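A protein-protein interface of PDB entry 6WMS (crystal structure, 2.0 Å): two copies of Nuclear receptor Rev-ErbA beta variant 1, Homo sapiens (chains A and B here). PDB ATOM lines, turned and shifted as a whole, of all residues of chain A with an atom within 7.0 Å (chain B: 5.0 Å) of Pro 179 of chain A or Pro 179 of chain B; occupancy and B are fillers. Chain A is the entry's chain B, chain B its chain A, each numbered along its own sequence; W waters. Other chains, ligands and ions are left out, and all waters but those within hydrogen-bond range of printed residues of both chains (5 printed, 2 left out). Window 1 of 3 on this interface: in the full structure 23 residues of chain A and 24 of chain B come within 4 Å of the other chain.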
ATOM      1  N   GLU A  64     -15.985  -8.597  10.448  1.00  0.00           N
ATOM      2  CA  GLU A  64     -15.853  -7.147  10.366  1.00  0.00           C
ATOM      3  C   GLU A  64     -16.270  -6.633   8.996  1.00  0.00           C
ATOM      4  O   GLU A  64     -16.850  -5.544   8.896  1.00  0.00           O
ATOM      5  CB  GLU A  64     -14.429  -6.723  10.725  1.00  0.00           C
ATOM      6  CG  GLU A  64     -14.049  -7.085  12.179  1.00  0.00           C
ATOM      7  CD  GLU A  64     -12.575  -6.831  12.517  1.00  0.00           C
ATOM      8  OE1 GLU A  64     -12.047  -5.762  12.140  1.00  0.00           O
ATOM      9  OE2 GLU A  64     -11.951  -7.695  13.170  1.00  0.00           O
ATOM     10  N   SER A 133      -6.884  -5.496   6.949  1.00  0.00           N
ATOM     11  CA  SER A 133      -6.397  -5.068   8.260  1.00  0.00           C
ATOM     12  C   SER A 133      -6.762  -6.042   9.383  1.00  0.00           C
ATOM     13  O   SER A 133      -6.533  -5.728  10.561  1.00  0.00           O
ATOM     14  CB  SER A 133      -6.937  -3.668   8.599  1.00  0.00           C
ATOM     15  OG  SER A 133      -6.522  -2.708   7.640  1.00  0.00           O
ATOM     16  N   ASP A 135      -6.827  -9.039  12.162  1.00  0.00           N
ATOM     17  CA  ASP A 135      -5.857  -9.555  13.127  1.00  0.00           C
ATOM     18  C   ASP A 135      -4.827 -10.430  12.424  1.00  0.00           C
ATOM     19  O   ASP A 135      -5.180 -11.347  11.684  1.00  0.00           O
ATOM     20  CB  ASP A 135      -6.612 -10.364  14.202  1.00  0.00           C
ATOM     21  CG  ASP A 135      -5.704 -10.907  15.306  1.00  0.00           C
ATOM     22  OD1 ASP A 135      -4.509 -10.556  15.370  1.00  0.00           O
ATOM     23  OD2 ASP A 135      -6.214 -11.695  16.136  1.00  0.00           O
ATOM     24  N   GLN A 149      -2.100  -4.046   2.756  1.00  0.00           N
ATOM     25  CA  GLN A 149      -2.838  -3.054   3.533  1.00  0.00           C
ATOM     26  C   GLN A 149      -2.419  -1.635   3.153  1.00  0.00           C
ATOM     27  O   GLN A 149      -3.261  -0.794   2.821  1.00  0.00           O
ATOM     28  CB  GLN A 149      -2.630  -3.303   5.029  1.00  0.00           C
ATOM     29  CG  GLN A 149      -3.291  -2.253   5.936  1.00  0.00           C
ATOM     30  CD  GLN A 149      -2.894  -2.423   7.391  1.00  0.00           C
ATOM     31  OE1 GLN A 149      -1.710  -2.509   7.713  1.00  0.00           O
ATOM     32  NE2 GLN A 149      -3.882  -2.520   8.271  1.00  0.00           N
ATOM     33  N   LEU A 174     -12.498   7.342   9.390  1.00  0.00           N
ATOM     34  CA  LEU A 174     -12.526   5.985   8.849  1.00  0.00           C
ATOM     35  C   LEU A 174     -11.483   5.104   9.510  1.00  0.00           C
ATOM     36  O   LEU A 174     -11.759   3.941   9.825  1.00  0.00           O
ATOM     37  CB  LEU A 174     -12.285   6.002   7.342  1.00  0.00           C
ATOM     38  CG  LEU A 174     -13.538   6.073   6.487  1.00  0.00           C
ATOM     39  CD1 LEU A 174     -13.145   5.914   5.023  1.00  0.00           C
ATOM     40  CD2 LEU A 174     -14.515   5.000   6.930  1.00  0.00           C
ATOM     41  N   LEU A 175     -10.270   5.629   9.706  1.00  0.00           N
ATOM     42  CA  LEU A 175      -9.239   4.839  10.374  1.00  0.00           C
ATOM     43  C   LEU A 175      -9.674   4.491  11.796  1.00  0.00           C
ATOM     44  O   LEU A 175      -9.405   3.388  12.288  1.00  0.00           O
ATOM     45  CB  LEU A 175      -7.907   5.599  10.381  1.00  0.00           C
ATOM     46  CG  LEU A 175      -7.070   5.771   9.093  1.00  0.00           C
ATOM     47  CD1 LEU A 175      -5.929   6.749   9.363  1.00  0.00           C
ATOM     48  CD2 LEU A 175      -6.493   4.455   8.533  1.00  0.00           C
ATOM     49  N   LEU A 176     -10.386   5.404  12.453  1.00  0.00           N
ATOM     50  CA  LEU A 176     -10.846   5.166  13.823  1.00  0.00           C
ATOM     51  C   LEU A 176     -11.963   4.131  13.922  1.00  0.00           C
ATOM     52  O   LEU A 176     -12.258   3.674  15.033  1.00  0.00           O
ATOM     53  CB  LEU A 176     -11.299   6.493  14.446  1.00  0.00           C
ATOM     54  CG  LEU A 176     -10.157   7.495  14.689  1.00  0.00           C
ATOM     55  CD1 LEU A 176     -10.682   8.886  15.090  1.00  0.00           C
ATOM     56  CD2 LEU A 176      -9.170   6.951  15.725  1.00  0.00           C
ATOM     57  N   LYS A 177     -12.605   3.764  12.805  1.00  0.00           N
ATOM     58  CA  LYS A 177     -13.549   2.644  12.806  1.00  0.00           C
ATOM     59  C   LYS A 177     -12.866   1.290  12.969  1.00  0.00           C
ATOM     60  O   LYS A 177     -13.521   0.340  13.399  1.00  0.00           O
ATOM     61  CB  LYS A 177     -14.377   2.597  11.504  1.00  0.00           C
ATOM     62  CG  LYS A 177     -15.089   3.904  11.140  1.00  0.00           C
ATOM     63  CD  LYS A 177     -16.313   4.113  12.008  1.00  0.00           C
ATOM     64  CE  LYS A 177     -16.749   5.585  12.047  1.00  0.00           C
ATOM     65  NZ  LYS A 177     -15.778   6.482  12.787  1.00  0.00           N
ATOM     66  N   LEU A 178     -11.578   1.159  12.615  1.00  0.00           N
ATOM     67  CA  LEU A 178     -10.958  -0.161  12.649  1.00  0.00           C
ATOM     68  C   LEU A 178     -10.830  -0.700  14.076  1.00  0.00           C
ATOM     69  O   LEU A 178     -11.158  -1.876  14.296  1.00  0.00           O
ATOM     70  CB  LEU A 178      -9.604  -0.148  11.925  1.00  0.00           C
ATOM     71  CG  LEU A 178      -9.616   0.339  10.469  1.00  0.00           C
ATOM     72  CD1 LEU A 178      -8.178   0.530   9.968  1.00  0.00           C
ATOM     73  CD2 LEU A 178     -10.455  -0.564   9.533  1.00  0.00           C
ATOM     74  N   PRO A 179     -10.352   0.079  15.061  1.00  0.00           N
ATOM     75  CA  PRO A 179     -10.380  -0.434  16.448  1.00  0.00           C
ATOM     76  C   PRO A 179     -11.786  -0.690  16.953  1.00  0.00           C
ATOM     77  O   PRO A 179     -11.983  -1.603  17.762  1.00  0.00           O
ATOM     78  CB  PRO A 179      -9.678   0.673  17.263  1.00  0.00           C
ATOM     79  CG  PRO A 179      -9.680   1.924  16.348  1.00  0.00           C
ATOM     80  CD  PRO A 179      -9.657   1.379  14.949  1.00  0.00           C
ATOM     81  N   ASP A 180     -12.763   0.099  16.508  1.00  0.00           N
ATOM     82  CA  ASP A 180     -14.140  -0.117  16.928  1.00  0.00           C
ATOM     83  C   ASP A 180     -14.659  -1.434  16.368  1.00  0.00           C
ATOM     84  O   ASP A 180     -15.276  -2.233  17.085  1.00  0.00           O
ATOM     85  CB  ASP A 180     -15.024   1.039  16.456  1.00  0.00           C
ATOM     86  CG  ASP A 180     -14.736   2.351  17.173  1.00  0.00           C
ATOM     87  OD1 ASP A 180     -13.915   2.365  18.127  1.00  0.00           O
ATOM     88  OD2 ASP A 180     -15.346   3.373  16.769  1.00  0.00           O
ATOM     89  N   LEU A 181     -14.409  -1.672  15.075  1.00  0.00           N
ATOM     90  CA  LEU A 181     -14.770  -2.948  14.468  1.00  0.00           C
ATOM     91  C   LEU A 181     -14.079  -4.097  15.169  1.00  0.00           C
ATOM     92  O   LEU A 181     -14.664  -5.174  15.339  1.00  0.00           O
ATOM     93  CB  LEU A 181     -14.393  -2.953  12.987  1.00  0.00           C
ATOM     94  CG  LEU A 181     -15.452  -2.375  12.057  1.00  0.00           C
ATOM     95  CD1 LEU A 181     -14.789  -1.999  10.748  1.00  0.00           C
ATOM     96  CD2 LEU A 181     -16.518  -3.430  11.842  1.00  0.00           C
ATOM     97  N   ARG A 182     -12.813  -3.905  15.547  1.00  0.00           N
ATOM     98  CA  ARG A 182     -12.087  -5.002  16.168  1.00  0.00           C
ATOM     99  C   ARG A 182     -12.695  -5.346  17.519  1.00  0.00           C
ATOM    100  O   ARG A 182     -12.771  -6.521  17.888  1.00  0.00           O
ATOM    101  CB  ARG A 182     -10.599  -4.656  16.309  1.00  0.00           C
ATOM    102  CG  ARG A 182      -9.739  -5.834  16.747  1.00  0.00           C
ATOM    103  CD  ARG A 182      -9.676  -6.894  15.631  1.00  0.00           C
ATOM    104  NE  ARG A 182      -9.548  -6.273  14.319  1.00  0.00           N
ATOM    105  CZ  ARG A 182      -8.389  -5.982  13.748  1.00  0.00           C
ATOM    106  NH1 ARG A 182      -7.254  -6.270  14.385  1.00  0.00           N
ATOM    107  NH2 ARG A 182      -8.369  -5.411  12.540  1.00  0.00           N
ATOM    108  N   SER A 183     -13.136  -4.327  18.269  1.00  0.00           N
ATOM    109  CA  SER A 183     -13.816  -4.592  19.533  1.00  0.00           C
ATOM    110  C   SER A 183     -15.178  -5.252  19.310  1.00  0.00           C
ATOM    111  O   SER A 183     -15.569  -6.116  20.089  1.00  0.00           O
ATOM    112  CB  SER A 183     -13.972  -3.298  20.336  1.00  0.00           C
ATOM    113  OG  SER A 183     -12.776  -3.003  21.056  1.00  0.00           O
ATOM    114  N   LEU A 184     -15.929  -4.829  18.284  1.00  0.00           N
ATOM    115  CA  LEU A 184     -17.176  -5.522  17.952  1.00  0.00           C
ATOM    116  C   LEU A 184     -16.910  -6.986  17.662  1.00  0.00           C
ATOM    117  O   LEU A 184     -17.638  -7.853  18.142  1.00  0.00           O
ATOM    118  CB  LEU A 184     -17.887  -4.877  16.751  1.00  0.00           C
ATOM    119  CG  LEU A 184     -18.352  -3.425  16.914  1.00  0.00           C
ATOM    120  CD1 LEU A 184     -18.908  -2.857  15.615  1.00  0.00           C
ATOM    121  CD2 LEU A 184     -19.389  -3.314  18.042  1.00  0.00           C
ATOM    122  N   ASN A 185     -15.841  -7.274  16.907  1.00  0.00           N
ATOM    123  CA  ASN A 185     -15.471  -8.648  16.567  1.00  0.00           C
ATOM    124  C   ASN A 185     -15.081  -9.448  17.806  1.00  0.00           C
ATOM    125  O   ASN A 185     -15.487 -10.607  17.964  1.00  0.00           O
ATOM    126  CB  ASN A 185     -14.317  -8.622  15.559  1.00  0.00           C
ATOM    127  CG  ASN A 185     -14.141  -9.935  14.822  1.00  0.00           C
ATOM    128  OD1 ASN A 185     -14.844 -10.908  15.083  1.00  0.00           O
ATOM    129  ND2 ASN A 185     -13.198  -9.962  13.885  1.00  0.00           N
ATOM    130  N   ASN A 186     -14.278  -8.845  18.696  1.00  0.00           N
ATOM    131  CA  ASN A 186     -13.882  -9.520  19.933  1.00  0.00           C
ATOM    132  C   ASN A 186     -15.098  -9.919  20.759  1.00  0.00           C
ATOM    133  O   ASN A 186     -15.204 -11.056  21.227  1.00  0.00           O
ATOM    134  CB  ASN A 186     -12.995  -8.602  20.773  1.00  0.00           C
ATOM    135  CG  ASN A 186     -11.602  -8.397  20.181  1.00  0.00           C
ATOM    136  OD1 ASN A 186     -11.146  -9.150  19.325  1.00  0.00           O
ATOM    137  ND2 ASN A 186     -10.925  -7.349  20.647  1.00  0.00           N
ATOM    138  N   LEU B 175      -2.320   5.492  13.552  1.00  0.00           N
ATOM    139  CA  LEU B 175      -3.703   5.090  13.801  1.00  0.00           C
ATOM    140  C   LEU B 175      -3.912   3.605  13.546  1.00  0.00           C
ATOM    141  O   LEU B 175      -4.738   2.971  14.214  1.00  0.00           O
ATOM    142  CB  LEU B 175      -4.658   5.915  12.938  1.00  0.00           C
ATOM    143  CG  LEU B 175      -5.312   7.091  13.680  1.00  0.00           C
ATOM    144  CD1 LEU B 175      -4.320   7.766  14.608  1.00  0.00           C
ATOM    145  CD2 LEU B 175      -5.857   8.082  12.702  1.00  0.00           C
ATOM    146  N   LEU B 176      -3.186   3.030  12.591  1.00  0.00           N
ATOM    147  CA  LEU B 176      -3.293   1.595  12.357  1.00  0.00           C
ATOM    148  C   LEU B 176      -2.748   0.779  13.521  1.00  0.00           C
ATOM    149  O   LEU B 176      -3.007  -0.420  13.572  1.00  0.00           O
ATOM    150  CB  LEU B 176      -2.576   1.199  11.071  1.00  0.00           C
ATOM    151  CG  LEU B 176      -3.308   1.584   9.775  1.00  0.00           C
ATOM    152  CD1 LEU B 176      -2.408   1.378   8.578  1.00  0.00           C
ATOM    153  CD2 LEU B 176      -4.572   0.767   9.611  1.00  0.00           C
ATOM    154  N   LYS B 177      -2.003   1.391  14.450  1.00  0.00           N
ATOM    155  CA  LYS B 177      -1.614   0.687  15.668  1.00  0.00           C
ATOM    156  C   LYS B 177      -2.808   0.407  16.571  1.00  0.00           C
ATOM    157  O   LYS B 177      -2.761  -0.530  17.383  1.00  0.00           O
ATOM    158  CB  LYS B 177      -0.594   1.499  16.459  1.00  0.00           C
ATOM    159  CG  LYS B 177       0.669   1.842  15.669  1.00  0.00           C
ATOM    160  CD  LYS B 177       1.527   0.603  15.459  1.00  0.00           C
ATOM    161  CE  LYS B 177       2.545   0.857  14.340  1.00  0.00           C
ATOM    162  NZ  LYS B 177       1.858   0.809  12.994  1.00  0.00           N
ATOM    163  N   LEU B 178      -3.857   1.226  16.482  1.00  0.00           N
ATOM    164  CA  LEU B 178      -4.992   1.065  17.385  1.00  0.00           C
ATOM    165  C   LEU B 178      -5.688  -0.289  17.240  1.00  0.00           C
ATOM    166  O   LEU B 178      -5.906  -0.952  18.265  1.00  0.00           O
ATOM    167  CB  LEU B 178      -5.976   2.226  17.210  1.00  0.00           C
ATOM    168  CG  LEU B 178      -5.428   3.624  17.548  1.00  0.00           C
ATOM    169  CD1 LEU B 178      -6.513   4.676  17.419  1.00  0.00           C
ATOM    170  CD2 LEU B 178      -4.850   3.656  18.965  1.00  0.00           C
ATOM    171  N   PRO B 179      -6.076  -0.739  16.031  1.00  0.00           N
ATOM    172  CA  PRO B 179      -6.663  -2.098  15.945  1.00  0.00           C
ATOM    173  C   PRO B 179      -5.664  -3.184  16.270  1.00  0.00           C
ATOM    174  O   PRO B 179      -6.044  -4.218  16.842  1.00  0.00           O
ATOM    175  CB  PRO B 179      -7.136  -2.200  14.488  1.00  0.00           C
ATOM    176  CG  PRO B 179      -6.373  -1.115  13.742  1.00  0.00           C
ATOM    177  CD  PRO B 179      -6.139  -0.023  14.744  1.00  0.00           C
ATOM    178  N   ASP B 180      -4.396  -2.982  15.910  1.00  0.00           N
ATOM    179  CA  ASP B 180      -3.346  -3.908  16.311  1.00  0.00           C
ATOM    180  C   ASP B 180      -3.329  -4.079  17.822  1.00  0.00           C
ATOM    181  O   ASP B 180      -3.275  -5.203  18.339  1.00  0.00           O
ATOM    182  CB  ASP B 180      -1.995  -3.385  15.843  1.00  0.00           C
ATOM    183  CG  ASP B 180      -1.787  -3.537  14.342  1.00  0.00           C
ATOM    184  OD1 ASP B 180      -2.721  -3.968  13.615  1.00  0.00           O
ATOM    185  OD2 ASP B 180      -0.663  -3.224  13.898  1.00  0.00           O
ATOM    186  N   LEU B 181      -3.344  -2.952  18.544  1.00  0.00           N
ATOM    187  CA  LEU B 181      -3.376  -2.998  20.003  1.00  0.00           C
ATOM    188  C   LEU B 181      -4.641  -3.686  20.509  1.00  0.00           C
ATOM    189  O   LEU B 181      -4.608  -4.406  21.513  1.00  0.00           O
ATOM    190  CB  LEU B 181      -3.285  -1.581  20.568  1.00  0.00           C
ATOM    191  CG  LEU B 181      -1.901  -0.960  20.688  1.00  0.00           C
ATOM    192  CD1 LEU B 181      -2.026   0.543  20.882  1.00  0.00           C
ATOM    193  CD2 LEU B 181      -1.186  -1.601  21.857  1.00  0.00           C
ATOM    194  N   ARG B 182      -5.771  -3.458  19.840  1.00  0.00           N
ATOM    195  CA  ARG B 182      -7.006  -4.097  20.276  1.00  0.00           C
ATOM    196  C   ARG B 182      -6.900  -5.617  20.169  1.00  0.00           C
ATOM    197  O   ARG B 182      -7.405  -6.349  21.030  1.00  0.00           O
ATOM    198  CB  ARG B 182      -8.182  -3.564  19.456  1.00  0.00           C
ATOM    199  CG  ARG B 182      -9.563  -3.695  20.154  1.00  0.00           C
ATOM    200  CD  ARG B 182      -9.561  -3.044  21.548  1.00  0.00           C
ATOM    201  NE  ARG B 182      -9.062  -1.679  21.520  1.00  0.00           N
ATOM    202  CZ  ARG B 182      -9.770  -0.621  21.132  1.00  0.00           C
ATOM    203  NH1 ARG B 182     -11.016  -0.770  20.710  1.00  0.00           N
ATOM    204  NH2 ARG B 182      -9.220   0.587  21.152  1.00  0.00           N
ATOM    205  N   SER B 183      -6.218  -6.111  19.132  1.00  0.00           N
ATOM    206  CA  SER B 183      -6.053  -7.553  18.982  1.00  0.00           C
ATOM    207  C   SER B 183      -5.080  -8.106  20.012  1.00  0.00           C
ATOM    208  O   SER B 183      -5.330  -9.163  20.607  1.00  0.00           O
ATOM    209  CB  SER B 183      -5.571  -7.879  17.570  1.00  0.00           C
ATOM    210  OG  SER B 183      -6.649  -7.719  16.668  1.00  0.00           O
HETATM  211  O   HOH W   1      -8.892  -9.494  17.615  1.00  0.00           O
HETATM  212  O   HOH W   2      -7.223 -11.262  19.319  1.00  0.00           O
HETATM  213  O   HOH W   3      -3.171  -2.531  11.515  1.00  0.00           O
HETATM  214  O   HOH W   4      -4.751  -5.365  12.997  1.00  0.00           O
HETATM  215  O   HOH W   5     -12.565   1.504  19.950  1.00  0.00           O
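Water W5 bridges the side-chain carboxylate (OD1) of Asp 180 of chain A (2.4 Å) and the guanidinium group (NH1) of Arg 182 of chain B (2.9 Å). Water W4 lies within hydrogen-bond range of the side-chain carboxylate (OD1) of Asp 180 of chain B (2.5 Å), the guanidinium group (NH1) of Arg 182 of chain A (3.0 Å) and the backbone carbonyl oxygen (O) of Ser 133 of chain A (3.0 Å). Water W3 lies within hydrogen-bond range of OD1 of Asp 180 of chain B (2.6 Å), O of Leu 176 of chain B (3.0 Å) and NE2 of Gln 149 of chain A (3.3 Å). Water W1 bridges OD1 of Asn 186 of chain A and OG of Ser 183 of chain B. Water W2 bridges O of Ser 183 of chain B (3.1 Å) and OD2 of Asp 135 of chain A (3.4 Å).
NE of Arg 182 of chain A is in salt-bridge range of OE2 of Glu 64 of chain A (3.0 Å). OG of Ser 133 of chain A is in hydrogen-bond range of NE2 of Gln 149 of chain A (2.7 Å). The backbone carbonyl oxygen (O) of Ser 133 of chain A sits at hydrogen-bond distance from the guanidinium group (NH2) of Arg 182 of chain A, at 2.7 Å. The backbone carbonyl oxygen (O) of Arg 182 of chain A sits close to the side-chain amide oxygen (OD1) of Asn 186 of chain A (3.4 Å).
Printed residues of chain B that touch a printed residue of chain A: Leu 175, Leu 176, Leu 178, Pro 179, Arg 182 and Ser 183. Hydrophobic or aromatic side chains of chain B within 4 Å of the printed part of chain A: Leu 175, Leu 176, Leu 178 and Pro 179. Of the 17 printed residues of chain A, 9 touch a printed residue of chain B. Hydrophobic or aromatic side chains of chain A within 4 Å of the printed part of chain B: Leu 175, Leu 176, Leu 178 and Pro 179. Among the printed residues, 14 pairs touch across the chains.
Asp 135 of chain A touches Ser 183 of chain B. Gln 149 of chain A touches Leu 176 of chain B (NE2 to CD2, 3.6 Å). CD2 of Leu 175 of chain B touches CD1 of Leu 175 of chain A (3.6 Å). Leu 178 of chain B touches Leu 176 of chain A (CD1 to CD2, 3.9 Å). Leu 176 of chain B touches Leu 178 of chain A (CD2 to CD1, 3.6 Å). CB of Leu 178 of chain A touches CG of Pro 179 of chain B (3.8 Å). CB of Leu 178 of chain B touches CG of Pro 179 of chain A, at 3.8 Å. Pro 179 of chain A touches Pro 179 of chain B (CD to CD, 3.8 Å). CG of Arg 182 of chain A touches CB of Arg 182 of chain B, at 3.9 Å. Arg 182 of chain B touches Asn 186 of chain A (O to ND2, 3.7 Å).
Leu 175 of chain B touches its own counterpart, Leu 175 of chain A. Leu 176 of chain A touches Leu 178 of chain B, and with the chains exchanged Leu 178 of chain A touches Leu 176 of chain B. Pro 179 of chain B touches its own counterpart, Pro 179 of chain A. Arg 182 of chain B touches its own counterpart, Arg 182 of chain A. Positions printed for both chains: 175, 176, 177, 178, 179, 180, 181, 182 and 183.
NH1 of Arg 182 of chain A is in hydrogen-bond range of O of Pro 179 of chain B. The guanidinium group (NH1) of Arg 182 of chain B lies within hydrogen-bond range of the backbone carbonyl oxygen (O) of Pro 179 of chain A (3.2 Å). NH1 of Arg 182 of chain B is in hydrogen-bond range of OG of Ser 183 of chain A, at 2.9 Å. The guanidinium group (NH1) of Arg 182 of chain A sits at hydrogen-bond distance from the side-chain hydroxyl (OG) of Ser 183 of chain B (2.8 Å).
Pro 179 of chain A touches three residues of chain B. Pro 179 of chain B touches three residues of chain A. Of the printed residues of chain B, Asp 135 of chain A touches Ser 183 (3.6 Å). Printed residues of chain B within 4 Å of Asn 186 of chain A: Arg 182. The nearest printed residue of chain B that does not touch Pro 179 of chain A is Leu 175 of chain B (5.2 Å). The nearest printed residue of chain B that does not touch Gln 149 of chain A is Asp 180 of chain B (5.7 Å).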
